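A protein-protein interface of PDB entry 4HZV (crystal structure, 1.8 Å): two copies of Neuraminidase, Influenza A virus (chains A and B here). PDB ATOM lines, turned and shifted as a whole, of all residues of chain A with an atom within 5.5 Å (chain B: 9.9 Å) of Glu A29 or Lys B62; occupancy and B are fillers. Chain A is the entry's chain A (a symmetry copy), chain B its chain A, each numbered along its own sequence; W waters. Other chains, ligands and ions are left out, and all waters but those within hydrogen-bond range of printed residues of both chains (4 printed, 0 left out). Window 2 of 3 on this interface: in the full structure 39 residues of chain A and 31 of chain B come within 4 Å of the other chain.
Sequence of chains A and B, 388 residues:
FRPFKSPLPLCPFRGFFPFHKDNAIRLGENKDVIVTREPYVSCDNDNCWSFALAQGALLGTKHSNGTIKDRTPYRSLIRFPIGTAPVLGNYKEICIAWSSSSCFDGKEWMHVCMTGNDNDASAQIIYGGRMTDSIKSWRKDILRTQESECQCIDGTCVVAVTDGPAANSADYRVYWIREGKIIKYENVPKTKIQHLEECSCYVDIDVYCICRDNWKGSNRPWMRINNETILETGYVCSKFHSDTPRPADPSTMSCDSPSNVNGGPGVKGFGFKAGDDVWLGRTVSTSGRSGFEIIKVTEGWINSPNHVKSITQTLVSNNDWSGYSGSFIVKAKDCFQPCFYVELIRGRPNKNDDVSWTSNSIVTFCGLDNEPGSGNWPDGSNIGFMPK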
ATOM      1  N   ALA A  24      22.712  -2.768  16.384  1.00  0.00           N
ATOM      2  CA  ALA A  24      21.817  -1.613  16.301  1.00  0.00           C
ATOM      3  C   ALA A  24      21.966  -0.813  15.012  1.00  0.00           C
ATOM      4  O   ALA A  24      20.987  -0.306  14.479  1.00  0.00           O
ATOM      5  CB  ALA A  24      22.005  -0.699  17.515  1.00  0.00           C
ATOM      6  N   ILE A  25      23.189  -0.685  14.507  1.00  0.00           N
ATOM      7  CA  ILE A  25      23.383   0.104  13.295  1.00  0.00           C
ATOM      8  C   ILE A  25      22.831  -0.633  12.066  1.00  0.00           C
ATOM      9  O   ILE A  25      22.100  -0.049  11.262  1.00  0.00           O
ATOM     10  CB  ILE A  25      24.861   0.502  13.105  1.00  0.00           C
ATOM     11  CG1 ILE A  25      25.382   1.220  14.359  1.00  0.00           C
ATOM     12  CG2 ILE A  25      25.021   1.382  11.878  1.00  0.00           C
ATOM     13  CD1 ILE A  25      24.657   2.512  14.691  1.00  0.00           C
ATOM     14  N   ARG A  26      23.172  -1.916  11.932  1.00  0.00           N
ATOM     15  CA  ARG A  26      22.569  -2.774  10.903  1.00  0.00           C
ATOM     16  C   ARG A  26      21.039  -2.664  10.908  1.00  0.00           C
ATOM     17  O   ARG A  26      20.409  -2.482   9.862  1.00  0.00           O
ATOM     18  CB  ARG A  26      22.980  -4.238  11.107  1.00  0.00           C
ATOM     19  CG  ARG A  26      24.465  -4.525  10.863  1.00  0.00           C
ATOM     20  CD  ARG A  26      24.857  -5.951  11.289  1.00  0.00           C
ATOM     21  NE  ARG A  26      23.995  -6.988  10.717  1.00  0.00           N
ATOM     22  CZ  ARG A  26      24.238  -7.636   9.582  1.00  0.00           C
ATOM     23  NH1 ARG A  26      23.390  -8.561   9.152  1.00  0.00           N
ATOM     24  NH2 ARG A  26      25.322  -7.361   8.873  1.00  0.00           N
ATOM     25  N   LEU A  27      20.443  -2.776  12.088  1.00  0.00           N
ATOM     26  CA  LEU A  27      18.986  -2.722  12.209  1.00  0.00           C
ATOM     27  C   LEU A  27      18.433  -1.306  12.010  1.00  0.00           C
ATOM     28  O   LEU A  27      17.222  -1.113  11.870  1.00  0.00           O
ATOM     29  CB  LEU A  27      18.549  -3.303  13.559  1.00  0.00           C
ATOM     30  CG  LEU A  27      18.796  -4.812  13.685  1.00  0.00           C
ATOM     31  CD1 LEU A  27      18.753  -5.297  15.128  1.00  0.00           C
ATOM     32  CD2 LEU A  27      17.776  -5.549  12.841  1.00  0.00           C
ATOM     33  N   GLY A  28      19.323  -0.318  11.976  1.00  0.00           N
ATOM     34  CA  GLY A  28      18.900   1.064  11.834  1.00  0.00           C
ATOM     35  C   GLY A  28      18.880   1.564  10.400  1.00  0.00           C
ATOM     36  O   GLY A  28      18.690   2.757  10.150  1.00  0.00           O
ATOM     37  N   GLU A  29      19.062   0.651   9.453  1.00  0.00           N
ATOM     38  CA  GLU A  29      19.180   1.027   8.050  1.00  0.00           C
ATOM     39  C   GLU A  29      17.921   1.726   7.546  1.00  0.00           C
ATOM     40  O   GLU A  29      17.996   2.605   6.688  1.00  0.00           O
ATOM     41  CB  GLU A  29      19.502  -0.198   7.182  1.00  0.00           C
ATOM     42  CG  GLU A  29      19.892   0.143   5.751  1.00  0.00           C
ATOM     43  CD  GLU A  29      19.835  -1.063   4.831  1.00  0.00           C
ATOM     44  OE1 GLU A  29      20.293  -2.149   5.241  1.00  0.00           O
ATOM     45  OE2 GLU A  29      19.315  -0.926   3.705  1.00  0.00           O
ATOM     46  N   ASN A  30      16.766   1.351   8.092  1.00  0.00           N
ATOM     47  CA  ASN A  30      15.495   1.937   7.664  1.00  0.00           C
ATOM     48  C   ASN A  30      14.997   3.051   8.590  1.00  0.00           C
ATOM     49  O   ASN A  30      13.809   3.376   8.596  1.00  0.00           O
ATOM     50  CB  ASN A  30      14.420   0.856   7.514  1.00  0.00           C
ATOM     51  CG  ASN A  30      13.293   1.278   6.583  1.00  0.00           C
ATOM     52  OD1 ASN A  30      12.112   1.087   6.884  1.00  0.00           O
ATOM     53  ND2 ASN A  30      13.654   1.868   5.449  1.00  0.00           N
ATOM     54  N   LYS A  31      15.907   3.612   9.381  1.00  0.00           N
ATOM     55  CA  LYS A  31      15.631   4.810  10.181  1.00  0.00           C
ATOM     56  C   LYS A  31      14.719   4.578  11.390  1.00  0.00           C
ATOM     57  O   LYS A  31      14.006   5.484  11.821  1.00  0.00           O
ATOM     58  CB  LYS A  31      15.065   5.929   9.295  1.00  0.00           C
ATOM     59  CG  LYS A  31      15.990   6.341   8.154  1.00  0.00           C
ATOM     60  CD  LYS A  31      15.381   7.448   7.304  1.00  0.00           C
ATOM     61  CE  LYS A  31      16.284   7.818   6.132  1.00  0.00           C
ATOM     62  NZ  LYS A  31      15.703   8.924   5.319  1.00  0.00           N
ATOM     63  N   GLY A 384      28.091   1.722   3.587  1.00  0.00           N
ATOM     64  CA  GLY A 384      27.607   2.108   2.276  1.00  0.00           C
ATOM     65  C   GLY A 384      26.119   1.878   2.102  1.00  0.00           C
ATOM     66  O   GLY A 384      25.489   2.509   1.257  1.00  0.00           O
ATOM     67  N   PHE A 385      25.554   0.975   2.900  1.00  0.00           N
ATOM     68  CA  PHE A 385      24.120   0.689   2.831  1.00  0.00           C
ATOM     69  C   PHE A 385      23.288   1.700   3.613  1.00  0.00           C
ATOM     70  O   PHE A 385      22.067   1.758   3.461  1.00  0.00           O
ATOM     71  CB  PHE A 385      23.817  -0.706   3.392  1.00  0.00           C
ATOM     72  CG  PHE A 385      24.305  -1.836   2.534  1.00  0.00           C
ATOM     73  CD1 PHE A 385      24.807  -1.607   1.265  1.00  0.00           C
ATOM     74  CD2 PHE A 385      24.252  -3.140   3.005  1.00  0.00           C
ATOM     75  CE1 PHE A 385      25.250  -2.661   0.480  1.00  0.00           C
ATOM     76  CE2 PHE A 385      24.694  -4.201   2.226  1.00  0.00           C
ATOM     77  CZ  PHE A 385      25.194  -3.961   0.963  1.00  0.00           C
ATOM     78  N   MET A 386      23.945   2.488   4.458  1.00  0.00           N
ATOM     79  CA  MET A 386      23.236   3.321   5.428  1.00  0.00           C
ATOM     80  C   MET A 386      22.791   4.666   4.874  1.00  0.00           C
ATOM     81  O   MET A 386      23.475   5.265   4.043  1.00  0.00           O
ATOM     82  CB  MET A 386      24.109   3.559   6.666  1.00  0.00           C
ATOM     83  CG  MET A 386      24.560   2.294   7.360  1.00  0.00           C
ATOM     84  SD  MET A 386      23.182   1.359   8.048  1.00  0.00           S
ATOM     85  CE  MET A 386      22.633   2.496   9.330  1.00  0.00           C
ATOM     86  N   PRO A 387      21.640   5.154   5.352  1.00  0.00           N
ATOM     87  CA  PRO A 387      21.255   6.541   5.081  1.00  0.00           C
ATOM     88  C   PRO A 387      22.305   7.451   5.713  1.00  0.00           C
ATOM     89  O   PRO A 387      22.739   7.183   6.836  1.00  0.00           O
ATOM     90  CB  PRO A 387      19.909   6.697   5.797  1.00  0.00           C
ATOM     91  CG  PRO A 387      19.778   5.529   6.705  1.00  0.00           C
ATOM     92  CD  PRO A 387      20.677   4.441   6.207  1.00  0.00           C
ATOM     93  N   ASN B  30       6.697  -3.998   4.338  1.00  0.00           N
ATOM     94  CA  ASN B  30       7.149  -2.617   4.505  1.00  0.00           C
ATOM     95  C   ASN B  30       8.419  -2.492   5.353  1.00  0.00           C
ATOM     96  O   ASN B  30       8.710  -1.425   5.893  1.00  0.00           O
ATOM     97  CB  ASN B  30       6.035  -1.747   5.096  1.00  0.00           C
ATOM     98  CG  ASN B  30       6.225  -0.268   4.793  1.00  0.00           C
ATOM     99  OD1 ASN B  30       6.073   0.587   5.669  1.00  0.00           O
ATOM    100  ND2 ASN B  30       6.574   0.039   3.548  1.00  0.00           N
ATOM    101  N   LYS B  31       9.155  -3.593   5.477  1.00  0.00           N
ATOM    102  CA  LYS B  31      10.487  -3.589   6.093  1.00  0.00           C
ATOM    103  C   LYS B  31      10.491  -3.411   7.614  1.00  0.00           C
ATOM    104  O   LYS B  31      11.449  -2.887   8.181  1.00  0.00           O
ATOM    105  CB  LYS B  31      11.382  -2.533   5.430  1.00  0.00           C
ATOM    106  CG  LYS B  31      11.569  -2.733   3.929  1.00  0.00           C
ATOM    107  CD  LYS B  31      12.458  -1.657   3.322  1.00  0.00           C
ATOM    108  CE  LYS B  31      12.597  -1.828   1.813  1.00  0.00           C
ATOM    109  NZ  LYS B  31      13.495  -0.795   1.223  1.00  0.00           N
ATOM    110  N   VAL B  35      14.792 -10.262  10.033  1.00  0.00           N
ATOM    111  CA  VAL B  35      15.130 -11.484   9.305  1.00  0.00           C
ATOM    112  C   VAL B  35      15.475 -12.601  10.283  1.00  0.00           C
ATOM    113  O   VAL B  35      16.288 -12.409  11.188  1.00  0.00           O
ATOM    114  CB  VAL B  35      16.343 -11.279   8.374  1.00  0.00           C
ATOM    115  CG1 VAL B  35      16.732 -12.600   7.741  1.00  0.00           C
ATOM    116  CG2 VAL B  35      16.030 -10.243   7.309  1.00  0.00           C
ATOM    117  N   GLN B  55      18.973 -12.477  12.050  1.00  0.00           N
ATOM    118  CA  GLN B  55      20.148 -12.275  11.205  1.00  0.00           C
ATOM    119  C   GLN B  55      20.684 -10.856  11.342  1.00  0.00           C
ATOM    120  O   GLN B  55      21.517 -10.410  10.541  1.00  0.00           O
ATOM    121  CB  GLN B  55      19.801 -12.563   9.743  1.00  0.00           C
ATOM    122  CG  GLN B  55      19.550 -14.031   9.445  1.00  0.00           C
ATOM    123  CD  GLN B  55      20.828 -14.788   9.140  1.00  0.00           C
ATOM    124  OE1 GLN B  55      21.926 -14.329   9.448  1.00  0.00           O
ATOM    125  NE2 GLN B  55      20.689 -15.958   8.530  1.00  0.00           N
ATOM    126  N   GLY B  56      20.222 -10.140  12.363  1.00  0.00           N
ATOM    127  CA  GLY B  56      20.752  -8.812  12.621  1.00  0.00           C
ATOM    128  C   GLY B  56      20.460  -7.843  11.492  1.00  0.00           C
ATOM    129  O   GLY B  56      21.259  -6.951  11.193  1.00  0.00           O
ATOM    130  N   ALA B  57      19.301  -8.009  10.871  1.00  0.00           N
ATOM    131  CA  ALA B  57      18.902  -7.163   9.756  1.00  0.00           C
ATOM    132  C   ALA B  57      17.394  -7.191   9.599  1.00  0.00           C
ATOM    133  O   ALA B  57      16.743  -8.170   9.968  1.00  0.00           O
ATOM    134  CB  ALA B  57      19.574  -7.631   8.462  1.00  0.00           C
ATOM    135  N   LEU B  58      16.848  -6.115   9.044  1.00  0.00           N
ATOM    136  CA  LEU B  58      15.432  -6.053   8.718  1.00  0.00           C
ATOM    137  C   LEU B  58      15.161  -6.591   7.316  1.00  0.00           C
ATOM    138  O   LEU B  58      15.887  -6.294   6.368  1.00  0.00           O
ATOM    139  CB  LEU B  58      14.913  -4.624   8.828  1.00  0.00           C
ATOM    140  CG  LEU B  58      14.916  -4.027  10.234  1.00  0.00           C
ATOM    141  CD1 LEU B  58      14.338  -2.618  10.205  1.00  0.00           C
ATOM    142  CD2 LEU B  58      14.139  -4.924  11.193  1.00  0.00           C
ATOM    143  N   LEU B  59      14.095  -7.369   7.206  1.00  0.00           N
ATOM    144  CA  LEU B  59      13.675  -7.987   5.946  1.00  0.00           C
ATOM    145  C   LEU B  59      13.468  -6.922   4.869  1.00  0.00           C
ATOM    146  O   LEU B  59      12.698  -5.976   5.055  1.00  0.00           O
ATOM    147  CB  LEU B  59      12.379  -8.768   6.187  1.00  0.00           C
ATOM    148  CG  LEU B  59      11.705  -9.676   5.143  1.00  0.00           C
ATOM    149  CD1 LEU B  59      11.396  -8.943   3.847  1.00  0.00           C
ATOM    150  CD2 LEU B  59      12.508 -10.932   4.885  1.00  0.00           C
ATOM    151  N   GLY B  60      14.162  -7.071   3.745  1.00  0.00           N
ATOM    152  CA  GLY B  60      13.978  -6.166   2.625  1.00  0.00           C
ATOM    153  C   GLY B  60      14.928  -4.983   2.612  1.00  0.00           C
ATOM    154  O   GLY B  60      14.900  -4.168   1.688  1.00  0.00           O
ATOM    155  N   THR B  61      15.767  -4.870   3.635  1.00  0.00           N
ATOM    156  CA  THR B  61      16.795  -3.839   3.620  1.00  0.00           C
ATOM    157  C   THR B  61      18.022  -4.411   2.930  1.00  0.00           C
ATOM    158  O   THR B  61      18.087  -5.608   2.654  1.00  0.00           O
ATOM    159  CB  THR B  61      17.172  -3.357   5.037  1.00  0.00           C
ATOM    160  OG1 THR B  61      17.796  -4.428   5.762  1.00  0.00           O
ATOM    161  CG2 THR B  61      15.939  -2.880   5.784  1.00  0.00           C
ATOM    162  N   LYS B  62      18.996  -3.558   2.642  1.00  0.00           N
ATOM    163  CA  LYS B  62      20.206  -4.011   1.974  1.00  0.00           C
ATOM    164  C   LYS B  62      20.968  -5.035   2.817  1.00  0.00           C
ATOM    165  O   LYS B  62      21.556  -5.977   2.281  1.00  0.00           O
ATOM    166  CB  LYS B  62      21.099  -2.822   1.616  1.00  0.00           C
ATOM    167  CG  LYS B  62      20.507  -1.892   0.566  1.00  0.00           C
ATOM    168  CD  LYS B  62      21.448  -0.735   0.259  1.00  0.00           C
ATOM    169  CE  LYS B  62      20.938   0.126  -0.886  1.00  0.00           C
ATOM    170  NZ  LYS B  62      19.641   0.763  -0.570  1.00  0.00           N
ATOM    171  N   HIS B  63      20.953  -4.856   4.137  1.00  0.00           N
ATOM    172  CA  HIS B  63      21.632  -5.791   5.035  1.00  0.00           C
ATOM    173  C   HIS B  63      21.000  -7.193   5.053  1.00  0.00           C
ATOM    174  O   HIS B  63      21.605  -8.138   5.544  1.00  0.00           O
ATOM    175  CB  HIS B  63      21.720  -5.235   6.467  1.00  0.00           C
ATOM    176  CG  HIS B  63      22.791  -4.207   6.658  1.00  0.00           C
ATOM    177  ND1 HIS B  63      22.561  -2.854   6.524  1.00  0.00           N
ATOM    178  CD2 HIS B  63      24.099  -4.336   6.988  1.00  0.00           C
ATOM    179  CE1 HIS B  63      23.684  -2.194   6.754  1.00  0.00           C
ATOM    180  NE2 HIS B  63      24.631  -3.071   7.040  1.00  0.00           N
ATOM    181  N   SER B  64      19.788  -7.331   4.523  1.00  0.00           N
ATOM    182  CA  SER B  64      19.140  -8.642   4.489  1.00  0.00           C
ATOM    183  C   SER B  64      19.643  -9.463   3.309  1.00  0.00           C
ATOM    184  O   SER B  64      19.445 -10.675   3.254  1.00  0.00           O
ATOM    185  CB  SER B  64      17.615  -8.515   4.427  1.00  0.00           C
ATOM    186  OG  SER B  64      17.184  -7.995   3.180  1.00  0.00           O
ATOM    187  N   ASN B  65      20.288  -8.788   2.365  1.00  0.00           N
ATOM    188  CA  ASN B  65      20.843  -9.439   1.181  1.00  0.00           C
ATOM    189  C   ASN B  65      21.881 -10.484   1.583  1.00  0.00           C
ATOM    190  O   ASN B  65      22.858 -10.164   2.250  1.00  0.00           O
ATOM    191  CB  ASN B  65      21.465  -8.377   0.266  1.00  0.00           C
ATOM    192  CG  ASN B  65      21.879  -8.925  -1.090  1.00  0.00           C
ATOM    193  OD1 ASN B  65      22.214 -10.106  -1.227  1.00  0.00           O
ATOM    194  ND2 ASN B  65      21.864  -8.055  -2.105  1.00  0.00           N
ATOM    195  N   GLY B  66      21.655 -11.738   1.200  1.00  0.00           N
ATOM    196  CA  GLY B  66      22.619 -12.793   1.469  1.00  0.00           C
ATOM    197  C   GLY B  66      22.455 -13.512   2.799  1.00  0.00           C
ATOM    198  O   GLY B  66      23.362 -14.234   3.250  1.00  0.00           O
ATOM    199  N   THR B  67      21.297 -13.334   3.430  1.00  0.00           N
ATOM    200  CA  THR B  67      21.029 -13.982   4.711  1.00  0.00           C
ATOM    201  C   THR B  67      20.766 -15.482   4.599  1.00  0.00           C
ATOM    202  O   THR B  67      20.329 -16.119   5.557  1.00  0.00           O
ATOM    203  CB  THR B  67      19.889 -13.289   5.491  1.00  0.00           C
ATOM    204  OG1 THR B  67      18.826 -12.947   4.594  1.00  0.00           O
ATOM    205  CG2 THR B  67      20.409 -12.020   6.150  1.00  0.00           C
ATOM    206  N   LEU B  88      11.279  -4.742  15.883  1.00  0.00           N
ATOM    207  CA  LEU B  88      12.150  -4.108  16.859  1.00  0.00           C
ATOM    208  C   LEU B  88      11.383  -3.699  18.112  1.00  0.00           C
ATOM    209  O   LEU B  88      11.939  -3.683  19.214  1.00  0.00           O
ATOM    210  CB  LEU B  88      12.859  -2.895  16.244  1.00  0.00           C
ATOM    211  CG  LEU B  88      13.804  -3.246  15.091  1.00  0.00           C
ATOM    212  CD1 LEU B  88      14.406  -1.991  14.473  1.00  0.00           C
ATOM    213  CD2 LEU B  88      14.888  -4.197  15.558  1.00  0.00           C
ATOM    214  N   SER B 356      16.751 -11.389  -2.535  1.00  0.00           N
ATOM    215  CA  SER B 356      18.142 -11.607  -2.160  1.00  0.00           C
ATOM    216  C   SER B 356      18.289 -12.131  -0.735  1.00  0.00           C
ATOM    217  O   SER B 356      19.372 -12.570  -0.340  1.00  0.00           O
ATOM    218  CB  SER B 356      18.955 -10.320  -2.327  1.00  0.00           C
ATOM    219  OG  SER B 356      18.685  -9.401  -1.281  1.00  0.00           O
ATOM    220  N   TRP B 357      17.199 -12.084   0.029  1.00  0.00           N
ATOM    221  CA  TRP B 357      17.227 -12.499   1.431  1.00  0.00           C
ATOM    222  C   TRP B 357      16.702 -13.913   1.641  1.00  0.00           C
ATOM    223  O   TRP B 357      16.195 -14.548   0.713  1.00  0.00           O
ATOM    224  CB  TRP B 357      16.444 -11.511   2.316  1.00  0.00           C
ATOM    225  CG  TRP B 357      15.103 -11.075   1.755  1.00  0.00           C
ATOM    226  CD1 TRP B 357      14.832  -9.902   1.117  1.00  0.00           C
ATOM    227  CD2 TRP B 357      13.865 -11.806   1.790  1.00  0.00           C
ATOM    228  NE1 TRP B 357      13.510  -9.852   0.752  1.00  0.00           N
ATOM    229  CE2 TRP B 357      12.892 -11.008   1.154  1.00  0.00           C
ATOM    230  CE3 TRP B 357      13.486 -13.057   2.294  1.00  0.00           C
ATOM    231  CZ2 TRP B 357      11.565 -11.417   1.007  1.00  0.00           C
ATOM    232  CZ3 TRP B 357      12.165 -13.461   2.147  1.00  0.00           C
ATOM    233  CH2 TRP B 357      11.223 -12.645   1.507  1.00  0.00           C
ATOM    234  N   THR B 358      16.849 -14.395   2.872  1.00  0.00           N
ATOM    235  CA  THR B 358      16.273 -15.661   3.307  1.00  0.00           C
ATOM    236  C   THR B 358      15.649 -15.459   4.681  1.00  0.00           C
ATOM    237  O   THR B 358      16.318 -15.011   5.606  1.00  0.00           O
ATOM    238  CB  THR B 358      17.338 -16.764   3.455  1.00  0.00           C
ATOM    239  OG1 THR B 358      17.910 -17.070   2.179  1.00  0.00           O
ATOM    240  CG2 THR B 358      16.703 -18.018   4.025  1.00  0.00           C
ATOM    241  N   PRO B 387       9.961  -6.429  -1.063  1.00  0.00           N
ATOM    242  CA  PRO B 387      11.250  -5.792  -1.338  1.00  0.00           C
ATOM    243  C   PRO B 387      12.298  -6.894  -1.476  1.00  0.00           C
ATOM    244  O   PRO B 387      12.282  -7.845  -0.692  1.00  0.00           O
ATOM    245  CB  PRO B 387      11.520  -4.950  -0.085  1.00  0.00           C
ATOM    246  CG  PRO B 387      10.565  -5.420   0.951  1.00  0.00           C
ATOM    247  CD  PRO B 387       9.419  -6.095   0.264  1.00  0.00           C
ATOM    248  N   LYS B 388      13.184  -6.777  -2.460  1.00  0.00           N
ATOM    249  CA  LYS B 388      14.136  -7.843  -2.753  1.00  0.00           C
ATOM    250  C   LYS B 388      15.424  -7.753  -1.932  1.00  0.00           C
ATOM    251  O   LYS B 388      15.728  -6.744  -1.297  1.00  0.00           O
ATOM    252  CB  LYS B 388      14.465  -7.872  -4.248  1.00  0.00           C
ATOM    253  CG  LYS B 388      13.258  -8.094  -5.154  1.00  0.00           C
ATOM    254  CD  LYS B 388      13.694  -8.281  -6.602  1.00  0.00           C
ATOM    255  CE  LYS B 388      12.508  -8.275  -7.549  1.00  0.00           C
ATOM    256  NZ  LYS B 388      11.527  -9.345  -7.225  1.00  0.00           N
ATOM    257  OXT LYS B 388      16.200  -8.708  -1.898  1.00  0.00           O
HETATM  258  O   HOH W   1       9.597   1.136   5.318  1.00  0.00           O
HETATM  259  O   HOH W   2      11.445  -0.182   9.141  1.00  0.00           O
HETATM  260  O   HOH W   3      23.964  -9.812   6.535  1.00  0.00           O
HETATM  261  O   HOH W   4      18.510  -3.904   8.337  1.00  0.00           O
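Water W2 lies within hydrogen-bond range of OD1 of Asn A30 (2.7 Å) and O of Lys B31 (2.9 Å).
Water W4 lies within hydrogen-bond range of OG1 of Thr B61, O of Arg A26 and N of Leu B58.
Water W1 lies within hydrogen-bond range of the backbone carbonyl oxygen (O) of Asn B30 and the side-chain amide oxygen (OD1) of Asn A30.
Water W3 lies within hydrogen-bond range of NH1 of Arg A26 and O of His B63.
The side-chain hydroxyl of Thr B61 lies close to the side-chain carboxylate of Glu A29.
The backbone NH (N) of Lys B62 sits at hydrogen-bond distance from the side-chain carboxylate (OE2) of Glu A29 (2.9 Å).
NE of Arg A26 sits at hydrogen-bond distance from O of Gly B56 (2.8 Å).
The backbone carbonyl oxygen (O) of Gln B55 sits at hydrogen-bond distance from the guanidinium group (NH1) of Arg A26 (3.0 Å).
A ring nitrogen (ND1) of His B63 is in hydrogen-bond range of the side-chain carboxylate (OE1) of Glu A29 (2.7 Å).
The backbone carbonyl oxygen (O) of Thr B67 is in hydrogen-bond range of the side-chain amide nitrogen (NE2) of Gln B55 (3.0 Å).
The backbone NH (N) of Val B35 sits at hydrogen-bond distance from the backbone carbonyl oxygen (O) of Ala B57 (2.9 Å).
OG of Ser B64 is in hydrogen-bond range of O of Thr B61 (2.6 Å).
The backbone NH (N) of Gln B55 sits at hydrogen-bond distance from the backbone carbonyl oxygen (O) of Val B35.
The side-chain hydroxyl (OG1) of Thr B61 lies within hydrogen-bond range of the backbone carbonyl oxygen (O) of Leu B58, at 2.7 Å.
No residue of chain B comes within 4 Å of Gly A28.
Glu A29 touches just these residues of chain B: Thr B61 (3.4 Å), Lys B62 (2.9 Å) and His B63 (2.7 Å).
Of the printed residues of chain A, Lys B31 touches Asn A30.
Printed residues of chain A within 4 Å of Thr B61: Glu A29 (3.4 Å).
Thr B358 touches none of the printed residues of chain A.
Of the 22 printed residues of chain B, 9 touch a printed residue of chain A.
Hydrophobic or aromatic side chains of chain B that line the printed part of chain A: Ala B57, Leu B58, His B63 and Leu B88.
Hydrophobic or aromatic side chains of chain A that line the printed part of chain B: Leu A27, Phe A385 and Met A386.
Among the printed residues, 15 pairs touch across the chains.
Among the printed residues, no Asp or Glu carboxylate lies within 4 Å of a Lys or Arg side-chain nitrogen of the other chain.
Arg A26 touches Ala B57 (NH1 to CB, 3.99 Å).
His B63 touches Arg A26 (CD2 to NH2, 3.8 Å).
Gly B56 touches Leu A27 (C to CD2, 3.8 Å).
Ala B57 touches Leu A27.
Leu A27 touches Leu B58.
Leu B88 touches Leu A27 (CD1 to O, 3.9 Å).
Asn A30 touches Lys B31.
Lys B62 touches Phe A385 (CB to CD2, 3.5 Å).
CB of Phe A385 touches CE1 of His B63 (3.7 Å).
Met A386 touches His B63.
Asn A30 touches Lys B31, but with the chains exchanged Lys A31 does not touch Asn B30 (9.5 Å).
Of the 15 pairs that touch across the chains among the printed residues, none has its exchanged pair printed and touching as well.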
